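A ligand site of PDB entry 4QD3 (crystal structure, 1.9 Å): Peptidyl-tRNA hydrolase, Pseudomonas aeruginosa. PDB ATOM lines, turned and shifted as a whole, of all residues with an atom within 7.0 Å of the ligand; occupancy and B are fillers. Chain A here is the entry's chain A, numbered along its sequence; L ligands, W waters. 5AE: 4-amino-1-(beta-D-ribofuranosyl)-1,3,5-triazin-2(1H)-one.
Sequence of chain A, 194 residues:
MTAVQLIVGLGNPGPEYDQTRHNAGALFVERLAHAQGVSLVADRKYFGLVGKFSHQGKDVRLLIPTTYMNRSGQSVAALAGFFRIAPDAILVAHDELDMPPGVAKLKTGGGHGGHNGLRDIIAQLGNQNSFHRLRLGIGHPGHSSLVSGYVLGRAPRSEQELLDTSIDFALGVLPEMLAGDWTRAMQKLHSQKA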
ATOM      1  N   ASN A  12     -28.753 -10.558 -10.036  1.00  0.00           N
ATOM      2  CA  ASN A  12     -30.056  -9.912  -9.881  1.00  0.00           C
ATOM      3  C   ASN A  12     -31.095 -10.950  -9.502  1.00  0.00           C
ATOM      4  O   ASN A  12     -31.035 -12.088  -9.964  1.00  0.00           O
ATOM      5  CB  ASN A  12     -30.470  -9.229 -11.182  1.00  0.00           C
ATOM      6  CG  ASN A  12     -29.780  -7.903 -11.388  1.00  0.00           C
ATOM      7  OD1 ASN A  12     -29.912  -6.984 -10.566  1.00  0.00           O
ATOM      8  ND2 ASN A  12     -29.053  -7.767 -12.494  1.00  0.00           N
ATOM      9  N   HIS A  22     -24.994 -11.727 -15.914  1.00  0.00           N
ATOM     10  CA  HIS A  22     -24.701 -10.906 -14.751  1.00  0.00           C
ATOM     11  C   HIS A  22     -24.863 -11.673 -13.434  1.00  0.00           C
ATOM     12  O   HIS A  22     -24.558 -11.157 -12.406  1.00  0.00           O
ATOM     13  CB  HIS A  22     -25.611  -9.675 -14.739  1.00  0.00           C
ATOM     14  CG  HIS A  22     -24.960  -8.415 -14.282  1.00  0.00           C
ATOM     15  ND1 HIS A  22     -23.609  -8.208 -14.297  1.00  0.00           N
ATOM     16  CD2 HIS A  22     -25.499  -7.258 -13.819  1.00  0.00           C
ATOM     17  CE1 HIS A  22     -23.338  -6.995 -13.871  1.00  0.00           C
ATOM     18  NE2 HIS A  22     -24.477  -6.395 -13.583  1.00  0.00           N
ATOM     19  N   MET A  69     -28.676  -5.689  -8.384  1.00  0.00           N
ATOM     20  CA  MET A  69     -27.215  -5.679  -8.478  1.00  0.00           C
ATOM     21  C   MET A  69     -26.630  -4.374  -7.937  1.00  0.00           C
ATOM     22  O   MET A  69     -25.698  -4.404  -7.129  1.00  0.00           O
ATOM     23  CB  MET A  69     -26.756  -5.877  -9.920  1.00  0.00           C
ATOM     24  CG  MET A  69     -25.257  -5.945 -10.083  1.00  0.00           C
ATOM     25  SD  MET A  69     -24.566  -7.386  -9.231  1.00  0.00           S
ATOM     26  CE  MET A  69     -24.690  -8.616 -10.537  1.00  0.00           C
ATOM     27  N   ASN A  70     -27.167  -3.236  -8.373  1.00  0.00           N
ATOM     28  CA  ASN A  70     -26.648  -1.931  -7.972  1.00  0.00           C
ATOM     29  C   ASN A  70     -26.799  -1.588  -6.483  1.00  0.00           C
ATOM     30  O   ASN A  70     -26.277  -0.563  -6.038  1.00  0.00           O
ATOM     31  CB  ASN A  70     -27.254  -0.816  -8.825  1.00  0.00           C
ATOM     32  CG  ASN A  70     -28.737  -0.649  -8.598  1.00  0.00           C
ATOM     33  OD1 ASN A  70     -29.491  -1.627  -8.652  1.00  0.00           O
ATOM     34  ND2 ASN A  70     -29.170   0.580  -8.352  1.00  0.00           N
ATOM     35  N   ASP A  95     -19.275 -11.784 -12.552  1.00  0.00           N
ATOM     36  CA  ASP A  95     -19.053 -11.866 -13.982  1.00  0.00           C
ATOM     37  C   ASP A  95     -18.026 -10.825 -14.429  1.00  0.00           C
ATOM     38  O   ASP A  95     -17.987  -9.708 -13.892  1.00  0.00           O
ATOM     39  CB  ASP A  95     -20.364 -11.639 -14.725  1.00  0.00           C
ATOM     40  CG  ASP A  95     -21.073 -10.371 -14.297  1.00  0.00           C
ATOM     41  OD1 ASP A  95     -21.305 -10.202 -13.074  1.00  0.00           O
ATOM     42  OD2 ASP A  95     -21.400  -9.558 -15.170  1.00  0.00           O
ATOM     43  N   LEU A  97     -16.485  -9.084 -17.905  1.00  0.00           N
ATOM     44  CA  LEU A  97     -16.498  -8.821 -19.346  1.00  0.00           C
ATOM     45  C   LEU A  97     -15.145  -9.007 -20.025  1.00  0.00           C
ATOM     46  O   LEU A  97     -15.077  -9.419 -21.184  1.00  0.00           O
ATOM     47  CB  LEU A  97     -16.974  -7.385 -19.615  1.00  0.00           C
ATOM     48  CG  LEU A  97     -18.457  -7.124 -19.285  1.00  0.00           C
ATOM     49  CD1 LEU A  97     -18.713  -5.651 -18.964  1.00  0.00           C
ATOM     50  CD2 LEU A  97     -19.337  -7.599 -20.416  1.00  0.00           C
ATOM     51  N   HIS A 112     -14.017  -1.150  -9.908  1.00  0.00           N
ATOM     52  CA  HIS A 112     -15.167  -1.893 -10.269  1.00  0.00           C
ATOM     53  C   HIS A 112     -15.344  -2.152 -11.736  1.00  0.00           C
ATOM     54  O   HIS A 112     -16.066  -3.018 -12.116  1.00  0.00           O
ATOM     55  CB  HIS A 112     -16.414  -1.241  -9.690  1.00  0.00           C
ATOM     56  CG  HIS A 112     -16.575   0.200 -10.087  1.00  0.00           C
ATOM     57  ND1 HIS A 112     -16.900   0.567 -11.308  1.00  0.00           N
ATOM     58  CD2 HIS A 112     -16.426   1.341  -9.364  1.00  0.00           C
ATOM     59  CE1 HIS A 112     -16.999   1.870 -11.362  1.00  0.00           C
ATOM     60  NE2 HIS A 112     -16.697   2.342 -10.176  1.00  0.00           N
ATOM     61  N   GLY A 113     -14.678  -1.381 -12.571  1.00  0.00           N
ATOM     62  CA  GLY A 113     -14.697  -1.588 -14.030  1.00  0.00           C
ATOM     63  C   GLY A 113     -16.041  -1.388 -14.721  1.00  0.00           C
ATOM     64  O   GLY A 113     -16.280  -1.901 -15.820  1.00  0.00           O
ATOM     65  N   GLY A 114     -16.919  -0.612 -14.100  1.00  0.00           N
ATOM     66  CA  GLY A 114     -18.308  -0.471 -14.567  1.00  0.00           C
ATOM     67  C   GLY A 114     -19.303  -1.491 -14.049  1.00  0.00           C
ATOM     68  O   GLY A 114     -20.474  -1.452 -14.418  1.00  0.00           O
ATOM     69  N   HIS A 115     -18.863  -2.425 -13.207  1.00  0.00           N
ATOM     70  CA  HIS A 115     -19.752  -3.415 -12.613  1.00  0.00           C
ATOM     71  C   HIS A 115     -20.437  -2.781 -11.410  1.00  0.00           C
ATOM     72  O   HIS A 115     -19.802  -2.505 -10.403  1.00  0.00           O
ATOM     73  CB  HIS A 115     -18.979  -4.662 -12.165  1.00  0.00           C
ATOM     74  CG  HIS A 115     -19.833  -5.866 -11.914  1.00  0.00           C
ATOM     75  ND1 HIS A 115     -20.729  -5.933 -10.863  1.00  0.00           N
ATOM     76  CD2 HIS A 115     -19.938  -7.049 -12.558  1.00  0.00           C
ATOM     77  CE1 HIS A 115     -21.355  -7.097 -10.893  1.00  0.00           C
ATOM     78  NE2 HIS A 115     -20.897  -7.793 -11.909  1.00  0.00           N
ATOM     79  N   ASN A 116     -21.746  -2.550 -11.519  1.00  0.00           N
ATOM     80  CA  ASN A 116     -22.470  -1.806 -10.487  1.00  0.00           C
ATOM     81  C   ASN A 116     -22.619  -2.530  -9.160  1.00  0.00           C
ATOM     82  O   ASN A 116     -22.779  -1.895  -8.130  1.00  0.00           O
ATOM     83  CB  ASN A 116     -23.829  -1.339 -11.009  1.00  0.00           C
ATOM     84  CG  ASN A 116     -23.700  -0.314 -12.112  1.00  0.00           C
ATOM     85  OD1 ASN A 116     -22.657   0.315 -12.281  1.00  0.00           O
ATOM     86  ND2 ASN A 116     -24.767  -0.131 -12.872  1.00  0.00           N
ATOM     87  N   GLY A 117     -22.547  -3.860  -9.183  1.00  0.00           N
ATOM     88  CA  GLY A 117     -22.460  -4.632  -7.948  1.00  0.00           C
ATOM     89  C   GLY A 117     -21.181  -4.351  -7.184  1.00  0.00           C
ATOM     90  O   GLY A 117     -21.216  -4.024  -5.987  1.00  0.00           O
ATOM     91  N   LEU A 118     -20.046  -4.484  -7.856  1.00  0.00           N
ATOM     92  CA  LEU A 118     -18.752  -4.208  -7.242  1.00  0.00           C
ATOM     93  C   LEU A 118     -18.680  -2.735  -6.771  1.00  0.00           C
ATOM     94  O   LEU A 118     -18.158  -2.453  -5.713  1.00  0.00           O
ATOM     95  CB  LEU A 118     -17.612  -4.488  -8.231  1.00  0.00           C
ATOM     96  CG  LEU A 118     -17.372  -5.953  -8.613  1.00  0.00           C
ATOM     97  CD1 LEU A 118     -16.304  -6.051  -9.695  1.00  0.00           C
ATOM     98  CD2 LEU A 118     -16.986  -6.769  -7.393  1.00  0.00           C
ATOM     99  N   ILE A 138     -17.204 -13.800 -18.900  1.00  0.00           N
ATOM    100  CA  ILE A 138     -18.432 -13.890 -19.668  1.00  0.00           C
ATOM    101  C   ILE A 138     -18.309 -13.356 -21.096  1.00  0.00           C
ATOM    102  O   ILE A 138     -19.288 -13.383 -21.861  1.00  0.00           O
ATOM    103  CB  ILE A 138     -19.603 -13.179 -18.954  1.00  0.00           C
ATOM    104  CG1 ILE A 138     -19.296 -11.698 -18.702  1.00  0.00           C
ATOM    105  CG2 ILE A 138     -19.938 -13.887 -17.655  1.00  0.00           C
ATOM    106  CD1 ILE A 138     -20.528 -10.838 -18.548  1.00  0.00           C
ATOM    107  N   HIS A 140     -17.091 -10.173 -23.935  1.00  0.00           N
ATOM    108  CA  HIS A 140     -17.508  -8.769 -24.156  1.00  0.00           C
ATOM    109  C   HIS A 140     -18.168  -8.693 -25.553  1.00  0.00           C
ATOM    110  O   HIS A 140     -17.630  -9.255 -26.504  1.00  0.00           O
ATOM    111  CB  HIS A 140     -16.285  -7.840 -24.079  1.00  0.00           C
ATOM    112  CG  HIS A 140     -16.625  -6.380 -23.955  1.00  0.00           C
ATOM    113  ND1 HIS A 140     -17.106  -5.640 -25.007  1.00  0.00           N
ATOM    114  CD2 HIS A 140     -16.539  -5.534 -22.900  1.00  0.00           C
ATOM    115  CE1 HIS A 140     -17.308  -4.400 -24.615  1.00  0.00           C
ATOM    116  NE2 HIS A 140     -16.972  -4.298 -23.341  1.00  0.00           N
ATOM    117  N   SER A 144     -19.285  -0.683 -26.100  1.00  0.00           N
ATOM    118  CA  SER A 144     -19.871  -0.249 -24.833  1.00  0.00           C
ATOM    119  C   SER A 144     -21.387  -0.173 -24.849  1.00  0.00           C
ATOM    120  O   SER A 144     -22.029  -0.480 -23.847  1.00  0.00           O
ATOM    121  CB  SER A 144     -19.308   1.126 -24.444  1.00  0.00           C
ATOM    122  OG  SER A 144     -19.659   2.091 -25.414  1.00  0.00           O
ATOM    123  N   VAL A 147     -23.158  -3.485 -23.927  1.00  0.00           N
ATOM    124  CA  VAL A 147     -22.831  -4.154 -22.656  1.00  0.00           C
ATOM    125  C   VAL A 147     -24.060  -4.419 -21.778  1.00  0.00           C
ATOM    126  O   VAL A 147     -24.231  -5.539 -21.275  1.00  0.00           O
ATOM    127  CB  VAL A 147     -21.756  -3.370 -21.857  1.00  0.00           C
ATOM    128  CG1 VAL A 147     -21.601  -3.923 -20.451  1.00  0.00           C
ATOM    129  CG2 VAL A 147     -20.432  -3.401 -22.597  1.00  0.00           C
ATOM    130  N   SER A 148     -24.922  -3.447 -21.631  1.00  0.00           N
ATOM    131  CA  SER A 148     -26.042  -3.608 -20.747  1.00  0.00           C
ATOM    132  C   SER A 148     -26.977  -4.736 -21.188  1.00  0.00           C
ATOM    133  O   SER A 148     -27.271  -5.590 -20.425  1.00  0.00           O
ATOM    134  CB  SER A 148     -26.761  -2.262 -20.620  1.00  0.00           C
ATOM    135  OG  SER A 148     -27.962  -2.371 -19.948  1.00  0.00           O
ATOM    136  N   GLY A 149     -27.335  -4.783 -22.451  1.00  0.00           N
ATOM    137  CA  GLY A 149     -28.145  -5.872 -22.980  1.00  0.00           C
ATOM    138  C   GLY A 149     -27.452  -7.223 -22.908  1.00  0.00           C
ATOM    139  O   GLY A 149     -28.092  -8.259 -22.697  1.00  0.00           O
ATOM    140  N   VAL A 151     -24.963  -8.332 -20.612  1.00  0.00           N
ATOM    141  CA  VAL A 151     -24.875  -8.917 -19.271  1.00  0.00           C
ATOM    142  C   VAL A 151     -26.257  -9.352 -18.746  1.00  0.00           C
ATOM    143  O   VAL A 151     -26.370 -10.334 -18.014  1.00  0.00           O
ATOM    144  CB  VAL A 151     -24.162  -8.006 -18.242  1.00  0.00           C
ATOM    145  CG1 VAL A 151     -22.785  -7.586 -18.755  1.00  0.00           C
ATOM    146  CG2 VAL A 151     -24.999  -6.793 -17.863  1.00  0.00           C
ATOM    147  N   LEU A 152     -27.302  -8.635 -19.153  1.00  0.00           N
ATOM    148  CA  LEU A 152     -28.679  -9.011 -18.815  1.00  0.00           C
ATOM    149  C   LEU A 152     -29.280 -10.055 -19.775  1.00  0.00           C
ATOM    150  O   LEU A 152     -30.453 -10.390 -19.644  1.00  0.00           O
ATOM    151  CB  LEU A 152     -29.562  -7.772 -18.767  1.00  0.00           C
ATOM    152  CG  LEU A 152     -29.161  -6.681 -17.769  1.00  0.00           C
ATOM    153  CD1 LEU A 152     -30.115  -5.485 -17.868  1.00  0.00           C
ATOM    154  CD2 LEU A 152     -29.119  -7.224 -16.360  1.00  0.00           C
HETATM  155  O2  5AE L   1     -21.005  -5.005 -15.607  1.00  0.00           O
HETATM  156  C2  5AE L   1     -21.079  -3.947 -16.260  1.00  0.00           C
HETATM  157  N3  5AE L   1     -19.939  -3.439 -16.780  1.00  0.00           N
HETATM  158  C4  5AE L   1     -19.977  -2.297 -17.479  1.00  0.00           C
HETATM  159  N4  5AE L   1     -18.830  -1.796 -17.988  1.00  0.00           N
HETATM  160  N5  5AE L   1     -21.163  -1.642 -17.668  1.00  0.00           N
HETATM  161  N1  5AE L   1     -22.266  -3.314 -16.445  1.00  0.00           N
HETATM  162  C6  5AE L   1     -22.289  -2.170 -17.152  1.00  0.00           C
HETATM  163  C1' 5AE L   1     -23.503  -3.871 -15.873  1.00  0.00           C
HETATM  164  O4' 5AE L   1     -24.572  -3.892 -16.827  1.00  0.00           O
HETATM  165  C4' 5AE L   1     -25.780  -3.972 -16.054  1.00  0.00           C
HETATM  166  C5' 5AE L   1     -27.000  -3.615 -16.898  1.00  0.00           C
HETATM  167  O5' 5AE L   1     -26.886  -2.280 -17.414  1.00  0.00           O
HETATM  168  C3' 5AE L   1     -25.534  -3.057 -14.856  1.00  0.00           C
HETATM  169  O3' 5AE L   1     -26.207  -3.511 -13.687  1.00  0.00           O
HETATM  170  C2' 5AE L   1     -24.019  -3.062 -14.685  1.00  0.00           C
HETATM  171  O2' 5AE L   1     -23.625  -3.645 -13.430  1.00  0.00           O
HETATM  172  O   HOH W   1     -15.977  -2.427 -19.140  1.00  0.00           O
HETATM  173  O   HOH W   2     -19.002  -0.400 -20.910  1.00  0.00           O
HETATM  174  O   HOH W   3     -21.540   0.883 -15.461  1.00  0.00           O
HETATM  175  O   HOH W   4     -17.061   0.984 -17.669  1.00  0.00           O
HETATM  176  O   HOH W   5     -28.227  -5.171 -13.157  1.00  0.00           O
HETATM  177  O   HOH W   6     -19.940   1.601 -17.998  1.00  0.00           O
HETATM  178  O   HOH W   7     -19.967  -7.351 -16.110  1.00  0.00           O
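N4 of the ligand sits at hydrogen-bond distance from O of Gly 113.
The backbone NH (N) of Asn 116 lies within hydrogen-bond range of an oxygen (O2') of the ligand, 2.9 Å away.
An oxygen (O5') of the ligand is in hydrogen-bond range of the side-chain hydroxyl of Ser 148.
A ring nitrogen (NE2) of His 22 sits at hydrogen-bond distance from an oxygen (O2') of the ligand (2.9 Å).
The backbone NH of His 22 is in hydrogen-bond range of the backbone carbonyl oxygen of Val 151.
The backbone NH (N) of Gly 117 is in hydrogen-bond range of a ring nitrogen (ND1) of His 115, 3.2 Å away.
The backbone carbonyl oxygen (O) of Leu 97 sits at hydrogen-bond distance from the backbone NH (N) of His 140 (3.5 Å).
The backbone NH (N) of Gly 114 sits at hydrogen-bond distance from a ring nitrogen (ND1) of His 112 (3.0 Å).
A ring nitrogen (ND1) of His 22 is in hydrogen-bond range of the side-chain carboxylate (OD2) of Asp 95.
A ring nitrogen (NE2) of His 115 lies within hydrogen-bond range of the side-chain carboxylate of Asp 95 (2.7 Å).
A ring nitrogen (ND1) of His 115 is in hydrogen-bond range of the backbone NH (N) of Leu 118, 3.4 Å away.
The backbone carbonyl oxygen of Gly 114 lies close to a nitrogen (N3) of the ligand (3.1 Å).
Leu 97 touches the ligand.
His 115 touches the ligand.
CG1 of Val 147 touches N5 of the ligand, at 3.6 Å.
Val 151 touches the ligand (CG2 to O4', 3.1 Å).
Leu 152 touches the ligand (CD1 to C5', 3.8 Å).
Hydrophobic or aromatic side chains that line the ligand: His 22, Leu 97, His 115, Val 147, Val 151 and Leu 152.
Within 4 Å of the ligand: His 22, Leu 97, Gly 113, Gly 114, His 115, Asn 116, Val 147, Ser 148, Val 151 and Leu 152.
The nearest printed residue that does not touch the ligand is Met 69 (4.4 Å).
Water W7 bridges an oxygen (O2) of the ligand and the side-chain carboxylate of Asp 95.
Water W5 lies within hydrogen-bond range of O3' of the ligand and ND2 of Asn 12.
Water W1 bridges a nitrogen (N4) of the ligand (3.1 Å) and the backbone carbonyl oxygen (O) of Gly 113 (3.4 Å).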
